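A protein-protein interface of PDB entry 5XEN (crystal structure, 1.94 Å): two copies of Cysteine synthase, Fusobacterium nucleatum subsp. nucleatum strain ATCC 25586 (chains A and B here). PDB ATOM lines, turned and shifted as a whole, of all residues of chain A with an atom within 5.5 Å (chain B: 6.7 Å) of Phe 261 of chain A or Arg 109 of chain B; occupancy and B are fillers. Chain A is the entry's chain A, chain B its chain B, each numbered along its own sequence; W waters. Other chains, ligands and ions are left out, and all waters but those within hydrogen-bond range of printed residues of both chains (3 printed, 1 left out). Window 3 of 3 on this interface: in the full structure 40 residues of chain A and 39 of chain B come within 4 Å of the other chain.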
ATOM      1  N   MET A 256     -26.656   5.227  28.098  1.00  0.00           N
ATOM      2  CA  MET A 256     -25.190   5.232  28.188  1.00  0.00           C
ATOM      3  C   MET A 256     -24.590   6.024  27.008  1.00  0.00           C
ATOM      4  O   MET A 256     -23.718   6.864  27.182  1.00  0.00           O
ATOM      5  CB  MET A 256     -24.697   3.784  28.236  1.00  0.00           C
ATOM      6  CG  MET A 256     -23.202   3.594  28.305  1.00  0.00           C
ATOM      7  SD  MET A 256     -22.709   1.835  28.385  1.00  0.00           S
ATOM      8  CE  MET A 256     -24.163   1.034  27.877  1.00  0.00           C
ATOM      9  N   ARG A 257     -25.101   5.772  25.811  1.00  0.00           N
ATOM     10  CA  ARG A 257     -24.636   6.469  24.605  1.00  0.00           C
ATOM     11  C   ARG A 257     -25.064   7.922  24.605  1.00  0.00           C
ATOM     12  O   ARG A 257     -24.280   8.779  24.163  1.00  0.00           O
ATOM     13  CB  ARG A 257     -25.179   5.803  23.341  1.00  0.00           C
ATOM     14  CG  ARG A 257     -24.526   4.484  23.013  1.00  0.00           C
ATOM     15  CD  ARG A 257     -25.088   3.822  21.737  1.00  0.00           C
ATOM     16  NE  ARG A 257     -24.984   2.359  21.854  1.00  0.00           N
ATOM     17  CZ  ARG A 257     -26.003   1.505  21.975  1.00  0.00           C
ATOM     18  NH1 ARG A 257     -27.266   1.945  21.962  1.00  0.00           N
ATOM     19  NH2 ARG A 257     -25.762   0.203  22.098  1.00  0.00           N
ATOM     20  N   GLU A 258     -26.283   8.222  25.071  1.00  0.00           N
ATOM     21  CA  GLU A 258     -26.698   9.619  25.139  1.00  0.00           C
ATOM     22  C   GLU A 258     -25.758  10.403  26.052  1.00  0.00           C
ATOM     23  O   GLU A 258     -25.388  11.540  25.752  1.00  0.00           O
ATOM     24  CB  GLU A 258     -28.145   9.810  25.612  1.00  0.00           C
ATOM     25  CG  GLU A 258     -28.669  11.140  25.129  1.00  0.00           C
ATOM     26  CD  GLU A 258     -30.167  11.329  25.292  1.00  0.00           C
ATOM     27  OE1 GLU A 258     -30.912  10.329  25.162  1.00  0.00           O
ATOM     28  OE2 GLU A 258     -30.594  12.480  25.532  1.00  0.00           O
ATOM     29  N   LEU A 259     -25.392   9.795  27.184  1.00  0.00           N
ATOM     30  CA  LEU A 259     -24.527  10.466  28.157  1.00  0.00           C
ATOM     31  C   LEU A 259     -23.151  10.782  27.559  1.00  0.00           C
ATOM     32  O   LEU A 259     -22.632  11.872  27.744  1.00  0.00           O
ATOM     33  CB  LEU A 259     -24.398   9.665  29.450  1.00  0.00           C
ATOM     34  CG  LEU A 259     -25.555   9.770  30.453  1.00  0.00           C
ATOM     35  CD1 LEU A 259     -25.469   8.639  31.477  1.00  0.00           C
ATOM     36  CD2 LEU A 259     -25.557  11.135  31.154  1.00  0.00           C
ATOM     37  N   SER A 260     -22.559   9.841  26.851  1.00  0.00           N
ATOM     38  CA  SER A 260     -21.252  10.076  26.274  1.00  0.00           C
ATOM     39  C   SER A 260     -21.358  11.063  25.092  1.00  0.00           C
ATOM     40  O   SER A 260     -20.545  11.986  24.996  1.00  0.00           O
ATOM     41  CB  SER A 260     -20.537   8.773  25.922  1.00  0.00           C
ATOM     42  OG  SER A 260     -21.289   7.960  25.031  1.00  0.00           O
ATOM     43  N   PHE A 261     -22.363  10.896  24.224  1.00  0.00           N
ATOM     44  CA  PHE A 261     -22.546  11.790  23.053  1.00  0.00           C
ATOM     45  C   PHE A 261     -22.834  13.237  23.421  1.00  0.00           C
ATOM     46  O   PHE A 261     -22.332  14.136  22.788  1.00  0.00           O
ATOM     47  CB  PHE A 261     -23.721  11.323  22.180  1.00  0.00           C
ATOM     48  CG  PHE A 261     -23.375  10.294  21.162  1.00  0.00           C
ATOM     49  CD1 PHE A 261     -22.384   9.355  21.375  1.00  0.00           C
ATOM     50  CD2 PHE A 261     -24.063  10.260  19.936  1.00  0.00           C
ATOM     51  CE1 PHE A 261     -22.065   8.400  20.430  1.00  0.00           C
ATOM     52  CE2 PHE A 261     -23.737   9.311  18.961  1.00  0.00           C
ATOM     53  CZ  PHE A 261     -22.741   8.362  19.223  1.00  0.00           C
ATOM     54  N   LYS A 262     -23.671  13.450  24.429  1.00  0.00           N
ATOM     55  CA  LYS A 262     -24.222  14.780  24.758  1.00  0.00           C
ATOM     56  C   LYS A 262     -23.578  15.458  25.951  1.00  0.00           C
ATOM     57  O   LYS A 262     -23.611  16.687  26.046  1.00  0.00           O
ATOM     58  CB  LYS A 262     -25.731  14.672  25.034  1.00  0.00           C
ATOM     59  CG  LYS A 262     -26.553  14.063  23.911  1.00  0.00           C
ATOM     60  CD  LYS A 262     -26.168  14.574  22.539  1.00  0.00           C
ATOM     61  CE  LYS A 262     -26.884  13.785  21.446  1.00  0.00           C
ATOM     62  NZ  LYS A 262     -26.534  14.296  20.087  1.00  0.00           N
ATOM     63  N   GLU A 263     -23.023  14.690  26.891  1.00  0.00           N
ATOM     64  CA  GLU A 263     -22.393  15.279  28.077  1.00  0.00           C
ATOM     65  C   GLU A 263     -20.891  14.991  28.211  1.00  0.00           C
ATOM     66  O   GLU A 263     -20.249  15.503  29.129  1.00  0.00           O
ATOM     67  CB  GLU A 263     -23.081  14.790  29.368  1.00  0.00           C
ATOM     68  CG  GLU A 263     -24.580  14.994  29.415  1.00  0.00           C
ATOM     69  CD  GLU A 263     -25.008  16.454  29.533  1.00  0.00           C
ATOM     70  OE1 GLU A 263     -24.294  17.246  30.185  1.00  0.00           O
ATOM     71  OE2 GLU A 263     -26.069  16.808  28.966  1.00  0.00           O
ATOM     72  N   GLY A 264     -20.335  14.167  27.330  1.00  0.00           N
ATOM     73  CA  GLY A 264     -18.967  13.727  27.473  1.00  0.00           C
ATOM     74  C   GLY A 264     -18.746  12.877  28.724  1.00  0.00           C
ATOM     75  O   GLY A 264     -17.626  12.799  29.240  1.00  0.00           O
ATOM     76  N   ALA B  82     -12.453  14.488  21.362  1.00  0.00           N
ATOM     77  CA  ALA B  82     -13.788  13.888  21.252  1.00  0.00           C
ATOM     78  C   ALA B  82     -14.677  14.199  22.437  1.00  0.00           C
ATOM     79  O   ALA B  82     -15.869  14.590  22.304  1.00  0.00           O
ATOM     80  CB  ALA B  82     -13.666  12.394  20.996  1.00  0.00           C
ATOM     81  N   CYS B  85     -15.465  17.977  22.435  1.00  0.00           N
ATOM     82  CA  CYS B  85     -16.421  18.241  21.363  1.00  0.00           C
ATOM     83  C   CYS B  85     -17.832  17.700  21.662  1.00  0.00           C
ATOM     84  O   CYS B  85     -18.854  18.315  21.248  1.00  0.00           O
ATOM     85  CB  CYS B  85     -15.888  17.721  20.045  1.00  0.00           C
ATOM     86  SG  CYS B  85     -14.477  18.650  19.380  1.00  0.00           S
ATOM     87  N   ALA B  86     -17.922  16.590  22.423  1.00  0.00           N
ATOM     88  CA  ALA B  86     -19.209  16.113  22.934  1.00  0.00           C
ATOM     89  C   ALA B  86     -19.847  17.151  23.851  1.00  0.00           C
ATOM     90  O   ALA B  86     -20.996  17.542  23.642  1.00  0.00           O
ATOM     91  CB  ALA B  86     -19.079  14.749  23.657  1.00  0.00           C
ATOM     92  N   VAL B  87     -19.095  17.680  24.799  1.00  0.00           N
ATOM     93  CA  VAL B  87     -19.612  18.693  25.717  1.00  0.00           C
ATOM     94  C   VAL B  87     -20.008  19.967  24.955  1.00  0.00           C
ATOM     95  O   VAL B  87     -21.058  20.574  25.245  1.00  0.00           O
ATOM     96  CB  VAL B  87     -18.576  19.060  26.793  1.00  0.00           C
ATOM     97  CG1 VAL B  87     -19.070  20.234  27.635  1.00  0.00           C
ATOM     98  CG2 VAL B  87     -18.247  17.837  27.652  1.00  0.00           C
ATOM     99  N   ASN B  89     -20.770  20.314  21.769  1.00  0.00           N
ATOM    100  CA  ASN B  89     -21.537  20.003  20.585  1.00  0.00           C
ATOM    101  C   ASN B  89     -20.841  20.399  19.272  1.00  0.00           C
ATOM    102  O   ASN B  89     -21.484  20.930  18.370  1.00  0.00           O
ATOM    103  CB  ASN B  89     -22.922  20.656  20.667  1.00  0.00           C
ATOM    104  CG  ASN B  89     -23.882  20.117  19.641  1.00  0.00           C
ATOM    105  OD1 ASN B  89     -23.868  18.925  19.295  1.00  0.00           O
ATOM    106  ND2 ASN B  89     -24.714  21.005  19.113  1.00  0.00           N
ATOM    107  N   ARG B 104      -8.818   2.818  21.432  1.00  0.00           N
ATOM    108  CA  ARG B 104      -8.773   4.234  21.078  1.00  0.00           C
ATOM    109  C   ARG B 104      -9.949   4.571  20.167  1.00  0.00           C
ATOM    110  O   ARG B 104     -10.632   5.562  20.388  1.00  0.00           O
ATOM    111  CB  ARG B 104      -7.489   4.598  20.355  1.00  0.00           C
ATOM    112  CG  ARG B 104      -6.286   4.683  21.247  1.00  0.00           C
ATOM    113  CD  ARG B 104      -5.012   4.469  20.418  1.00  0.00           C
ATOM    114  NE  ARG B 104      -3.879   5.107  21.061  1.00  0.00           N
ATOM    115  CZ  ARG B 104      -3.341   4.720  22.205  1.00  0.00           C
ATOM    116  NH1 ARG B 104      -3.828   3.672  22.851  1.00  0.00           N
ATOM    117  NH2 ARG B 104      -2.315   5.406  22.723  1.00  0.00           N
ATOM    118  N   ILE B 105     -10.172   3.723  19.159  1.00  0.00           N
ATOM    119  CA  ILE B 105     -11.282   3.922  18.244  1.00  0.00           C
ATOM    120  C   ILE B 105     -12.609   3.874  18.998  1.00  0.00           C
ATOM    121  O   ILE B 105     -13.472   4.714  18.806  1.00  0.00           O
ATOM    122  CB  ILE B 105     -11.323   2.865  17.126  1.00  0.00           C
ATOM    123  CG1 ILE B 105     -10.059   2.910  16.261  1.00  0.00           C
ATOM    124  CG2 ILE B 105     -12.600   3.030  16.306  1.00  0.00           C
ATOM    125  CD1 ILE B 105      -9.837   1.669  15.404  1.00  0.00           C
ATOM    126  N   GLN B 106     -12.764   2.881  19.856  1.00  0.00           N
ATOM    127  CA  GLN B 106     -14.028   2.679  20.551  1.00  0.00           C
ATOM    128  C   GLN B 106     -14.327   3.868  21.477  1.00  0.00           C
ATOM    129  O   GLN B 106     -15.481   4.284  21.615  1.00  0.00           O
ATOM    130  CB  GLN B 106     -14.008   1.388  21.370  1.00  0.00           C
ATOM    131  CG  GLN B 106     -13.719   0.103  20.612  1.00  0.00           C
ATOM    132  CD  GLN B 106     -14.851  -0.359  19.749  1.00  0.00           C
ATOM    133  OE1 GLN B 106     -15.392   0.389  18.941  1.00  0.00           O
ATOM    134  NE2 GLN B 106     -15.235  -1.629  19.926  1.00  0.00           N
ATOM    135  N   LEU B 107     -13.294   4.397  22.120  1.00  0.00           N
ATOM    136  CA  LEU B 107     -13.483   5.558  22.991  1.00  0.00           C
ATOM    137  C   LEU B 107     -13.904   6.781  22.184  1.00  0.00           C
ATOM    138  O   LEU B 107     -14.870   7.441  22.533  1.00  0.00           O
ATOM    139  CB  LEU B 107     -12.242   5.831  23.806  1.00  0.00           C
ATOM    140  CG  LEU B 107     -11.976   4.802  24.925  1.00  0.00           C
ATOM    141  CD1 LEU B 107     -10.528   4.892  25.448  1.00  0.00           C
ATOM    142  CD2 LEU B 107     -12.971   4.984  26.068  1.00  0.00           C
ATOM    143  N   MET B 108     -13.200   7.054  21.091  1.00  0.00           N
ATOM    144  CA  MET B 108     -13.559   8.203  20.260  1.00  0.00           C
ATOM    145  C   MET B 108     -14.989   8.071  19.731  1.00  0.00           C
ATOM    146  O   MET B 108     -15.763   9.034  19.770  1.00  0.00           O
ATOM    147  CB  MET B 108     -12.567   8.373  19.108  1.00  0.00           C
ATOM    148  CG  MET B 108     -11.275   9.032  19.585  1.00  0.00           C
ATOM    149  SD  MET B 108     -10.163   9.329  18.207  1.00  0.00           S
ATOM    150  CE  MET B 108      -9.353   7.764  18.087  1.00  0.00           C
ATOM    151  N   ARG B 109     -15.339   6.887  19.233  1.00  0.00           N
ATOM    152  CA  ARG B 109     -16.703   6.658  18.715  1.00  0.00           C
ATOM    153  C   ARG B 109     -17.781   6.754  19.796  1.00  0.00           C
ATOM    154  O   ARG B 109     -18.856   7.245  19.524  1.00  0.00           O
ATOM    155  CB  ARG B 109     -16.785   5.344  17.953  1.00  0.00           C
ATOM    156  CG  ARG B 109     -15.925   5.361  16.683  1.00  0.00           C
ATOM    157  CD  ARG B 109     -16.146   4.092  15.914  1.00  0.00           C
ATOM    158  NE  ARG B 109     -17.311   4.264  15.094  1.00  0.00           N
ATOM    159  CZ  ARG B 109     -18.054   3.294  14.565  1.00  0.00           C
ATOM    160  NH1 ARG B 109     -17.812   2.020  14.850  1.00  0.00           N
ATOM    161  NH2 ARG B 109     -19.092   3.608  13.816  1.00  0.00           N
ATOM    162  N   ALA B 110     -17.467   6.367  21.031  1.00  0.00           N
ATOM    163  CA  ALA B 110     -18.408   6.498  22.165  1.00  0.00           C
ATOM    164  C   ALA B 110     -18.800   7.954  22.369  1.00  0.00           C
ATOM    165  O   ALA B 110     -19.898   8.238  22.796  1.00  0.00           O
ATOM    166  CB  ALA B 110     -17.777   5.963  23.450  1.00  0.00           C
ATOM    167  N   TYR B 111     -17.877   8.878  22.103  1.00  0.00           N
ATOM    168  CA  TYR B 111     -18.153  10.315  22.228  1.00  0.00           C
ATOM    169  C   TYR B 111     -18.742  10.931  20.951  1.00  0.00           C
ATOM    170  O   TYR B 111     -19.010  12.126  20.918  1.00  0.00           O
ATOM    171  CB  TYR B 111     -16.865  11.077  22.579  1.00  0.00           C
ATOM    172  CG  TYR B 111     -16.346  10.779  23.960  1.00  0.00           C
ATOM    173  CD1 TYR B 111     -17.094  11.104  25.090  1.00  0.00           C
ATOM    174  CD2 TYR B 111     -15.104  10.205  24.149  1.00  0.00           C
ATOM    175  CE1 TYR B 111     -16.611  10.844  26.369  1.00  0.00           C
ATOM    176  CE2 TYR B 111     -14.618   9.946  25.422  1.00  0.00           C
ATOM    177  CZ  TYR B 111     -15.379  10.265  26.524  1.00  0.00           C
ATOM    178  OH  TYR B 111     -14.879   9.984  27.790  1.00  0.00           O
ATOM    179  N   GLY B 112     -18.925  10.128  19.901  1.00  0.00           N
ATOM    180  CA  GLY B 112     -19.576  10.606  18.671  1.00  0.00           C
ATOM    181  C   GLY B 112     -18.618  11.051  17.588  1.00  0.00           C
ATOM    182  O   GLY B 112     -19.038  11.616  16.595  1.00  0.00           O
ATOM    183  N   THR B 113     -17.343  10.731  17.740  1.00  0.00           N
ATOM    184  CA  THR B 113     -16.307  11.164  16.819  1.00  0.00           C
ATOM    185  C   THR B 113     -16.202  10.192  15.661  1.00  0.00           C
ATOM    186  O   THR B 113     -16.301   8.971  15.849  1.00  0.00           O
ATOM    187  CB  THR B 113     -14.948  11.349  17.554  1.00  0.00           C
ATOM    188  OG1 THR B 113     -15.049  12.588  18.314  1.00  0.00           O
ATOM    189  CG2 THR B 113     -13.813  11.419  16.527  1.00  0.00           C
ATOM    190  N   GLU B 114     -16.044  10.718  14.453  1.00  0.00           N
ATOM    191  CA  GLU B 114     -15.749   9.874  13.299  1.00  0.00           C
ATOM    192  C   GLU B 114     -14.259   9.661  13.125  1.00  0.00           C
ATOM    193  O   GLU B 114     -13.460  10.627  13.219  1.00  0.00           O
ATOM    194  CB  GLU B 114     -16.338  10.416  11.999  1.00  0.00           C
ATOM    195  CG  GLU B 114     -17.850  10.452  12.018  1.00  0.00           C
ATOM    196  CD  GLU B 114     -18.432  10.698  10.644  1.00  0.00           C
ATOM    197  OE1 GLU B 114     -18.437   9.745   9.827  1.00  0.00           O
ATOM    198  OE2 GLU B 114     -18.877  11.841  10.389  1.00  0.00           O
ATOM    199  N   VAL B 115     -13.893   8.416  12.807  1.00  0.00           N
ATOM    200  CA  VAL B 115     -12.501   8.024  12.654  1.00  0.00           C
ATOM    201  C   VAL B 115     -12.185   7.597  11.221  1.00  0.00           C
ATOM    202  O   VAL B 115     -12.886   6.787  10.647  1.00  0.00           O
ATOM    203  CB  VAL B 115     -12.146   6.870  13.604  1.00  0.00           C
ATOM    204  CG1 VAL B 115     -10.671   6.488  13.457  1.00  0.00           C
ATOM    205  CG2 VAL B 115     -12.463   7.282  15.040  1.00  0.00           C
HETATM  206  O   HOH W   1     -23.993  18.091  23.581  1.00  0.00           O
HETATM  207  O   HOH W   2     -20.922  13.949  20.511  1.00  0.00           O
HETATM  208  O   HOH W   3     -16.238  10.882  30.243  1.00  0.00           O
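Printed residues of chain B within 4 Å of Phe 261 of chain A: Ala 86, Arg 109, Ala 110, Tyr 111 and Gly 112.
Arg 109 of chain B touches one residue of chain A.
Printed residues of chain B within 4 Å of Ser 260 of chain A: Ala 86, Ala 110 and Tyr 111.
Of the printed residues of chain B, Lys 262 of chain A touches Ala 86.
The nearest printed residue of chain B that does not touch Phe 261 of chain A is Val 87 of chain B (5.2 Å).
The nearest printed residue of chain A that does not touch Arg 109 of chain B is Ser 260 of chain A (6.1 Å).
No position is printed for both chains.
Ala 86 of chain B touches Ser 260 of chain A.
Phe 261 of chain A touches Ala 86 of chain B (O to CB, 3.4 Å).
Arg 109 of chain B touches Phe 261 of chain A (O to CE1, 3.5 Å).
CD1 of Phe 261 of chain A touches O of Ala 110 of chain B (3.1 Å).
Phe 261 of chain A touches Tyr 111 of chain B (CD1 to C, 3.99 Å).
CE1 of Phe 261 of chain A touches N of Gly 112 of chain B, 3.6 Å away.
O of Lys 262 of chain A touches O of Ala 86 of chain B, at 3.7 Å.
O of Glu 263 of chain A touches CG2 of Val 87 of chain B, 3.4 Å away.
Ala 86 of chain B touches Gly 264 of chain A.
O of Gly 264 of chain A touches CE1 of Tyr 111 of chain B, at 3.6 Å.
Water W3 lies within hydrogen-bond range of the backbone carbonyl oxygen of Gly 264 of chain A and the side-chain hydroxyl of Tyr 111 of chain B.
Water W2 bridges the backbone carbonyl oxygen of Tyr 111 of chain B (2.7 Å) and the backbone carbonyl oxygen of Phe 261 of chain A (2.7 Å).
Water W1 lies within hydrogen-bond range of the backbone carbonyl oxygen (O) of Lys 262 of chain A and the backbone carbonyl oxygen (O) of Ala 86 of chain B.
The backbone carbonyl oxygen of Met 256 of chain A lies within hydrogen-bond range of the side-chain hydroxyl of Ser 260 of chain A, at 3.4 Å.
O of Arg 257 of chain A is in hydrogen-bond range of OG of Ser 260 of chain A, at 3.2 Å.
The backbone NH (N) of Gly 264 of chain A is in hydrogen-bond range of the backbone carbonyl oxygen (O) of Leu 259 of chain A, 3.3 Å away.
OG of Ser 260 of chain A lies within hydrogen-bond range of O of Ala 110 of chain B (2.6 Å).
Hydrophobic or aromatic side chains of chain A that line the printed part of chain B: Phe 261.
Of the 17 printed residues of chain B, 6 touch a printed residue of chain A.
Hydrophobic or aromatic side chains of chain B that line the printed part of chain A: Ala 86, Val 87 and Tyr 111.
Among the printed residues, 12 pairs touch across the chains.
Among the printed residues, no Asp or Glu carboxylate lies within 4 Å of a Lys or Arg side-chain nitrogen of the other chain.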
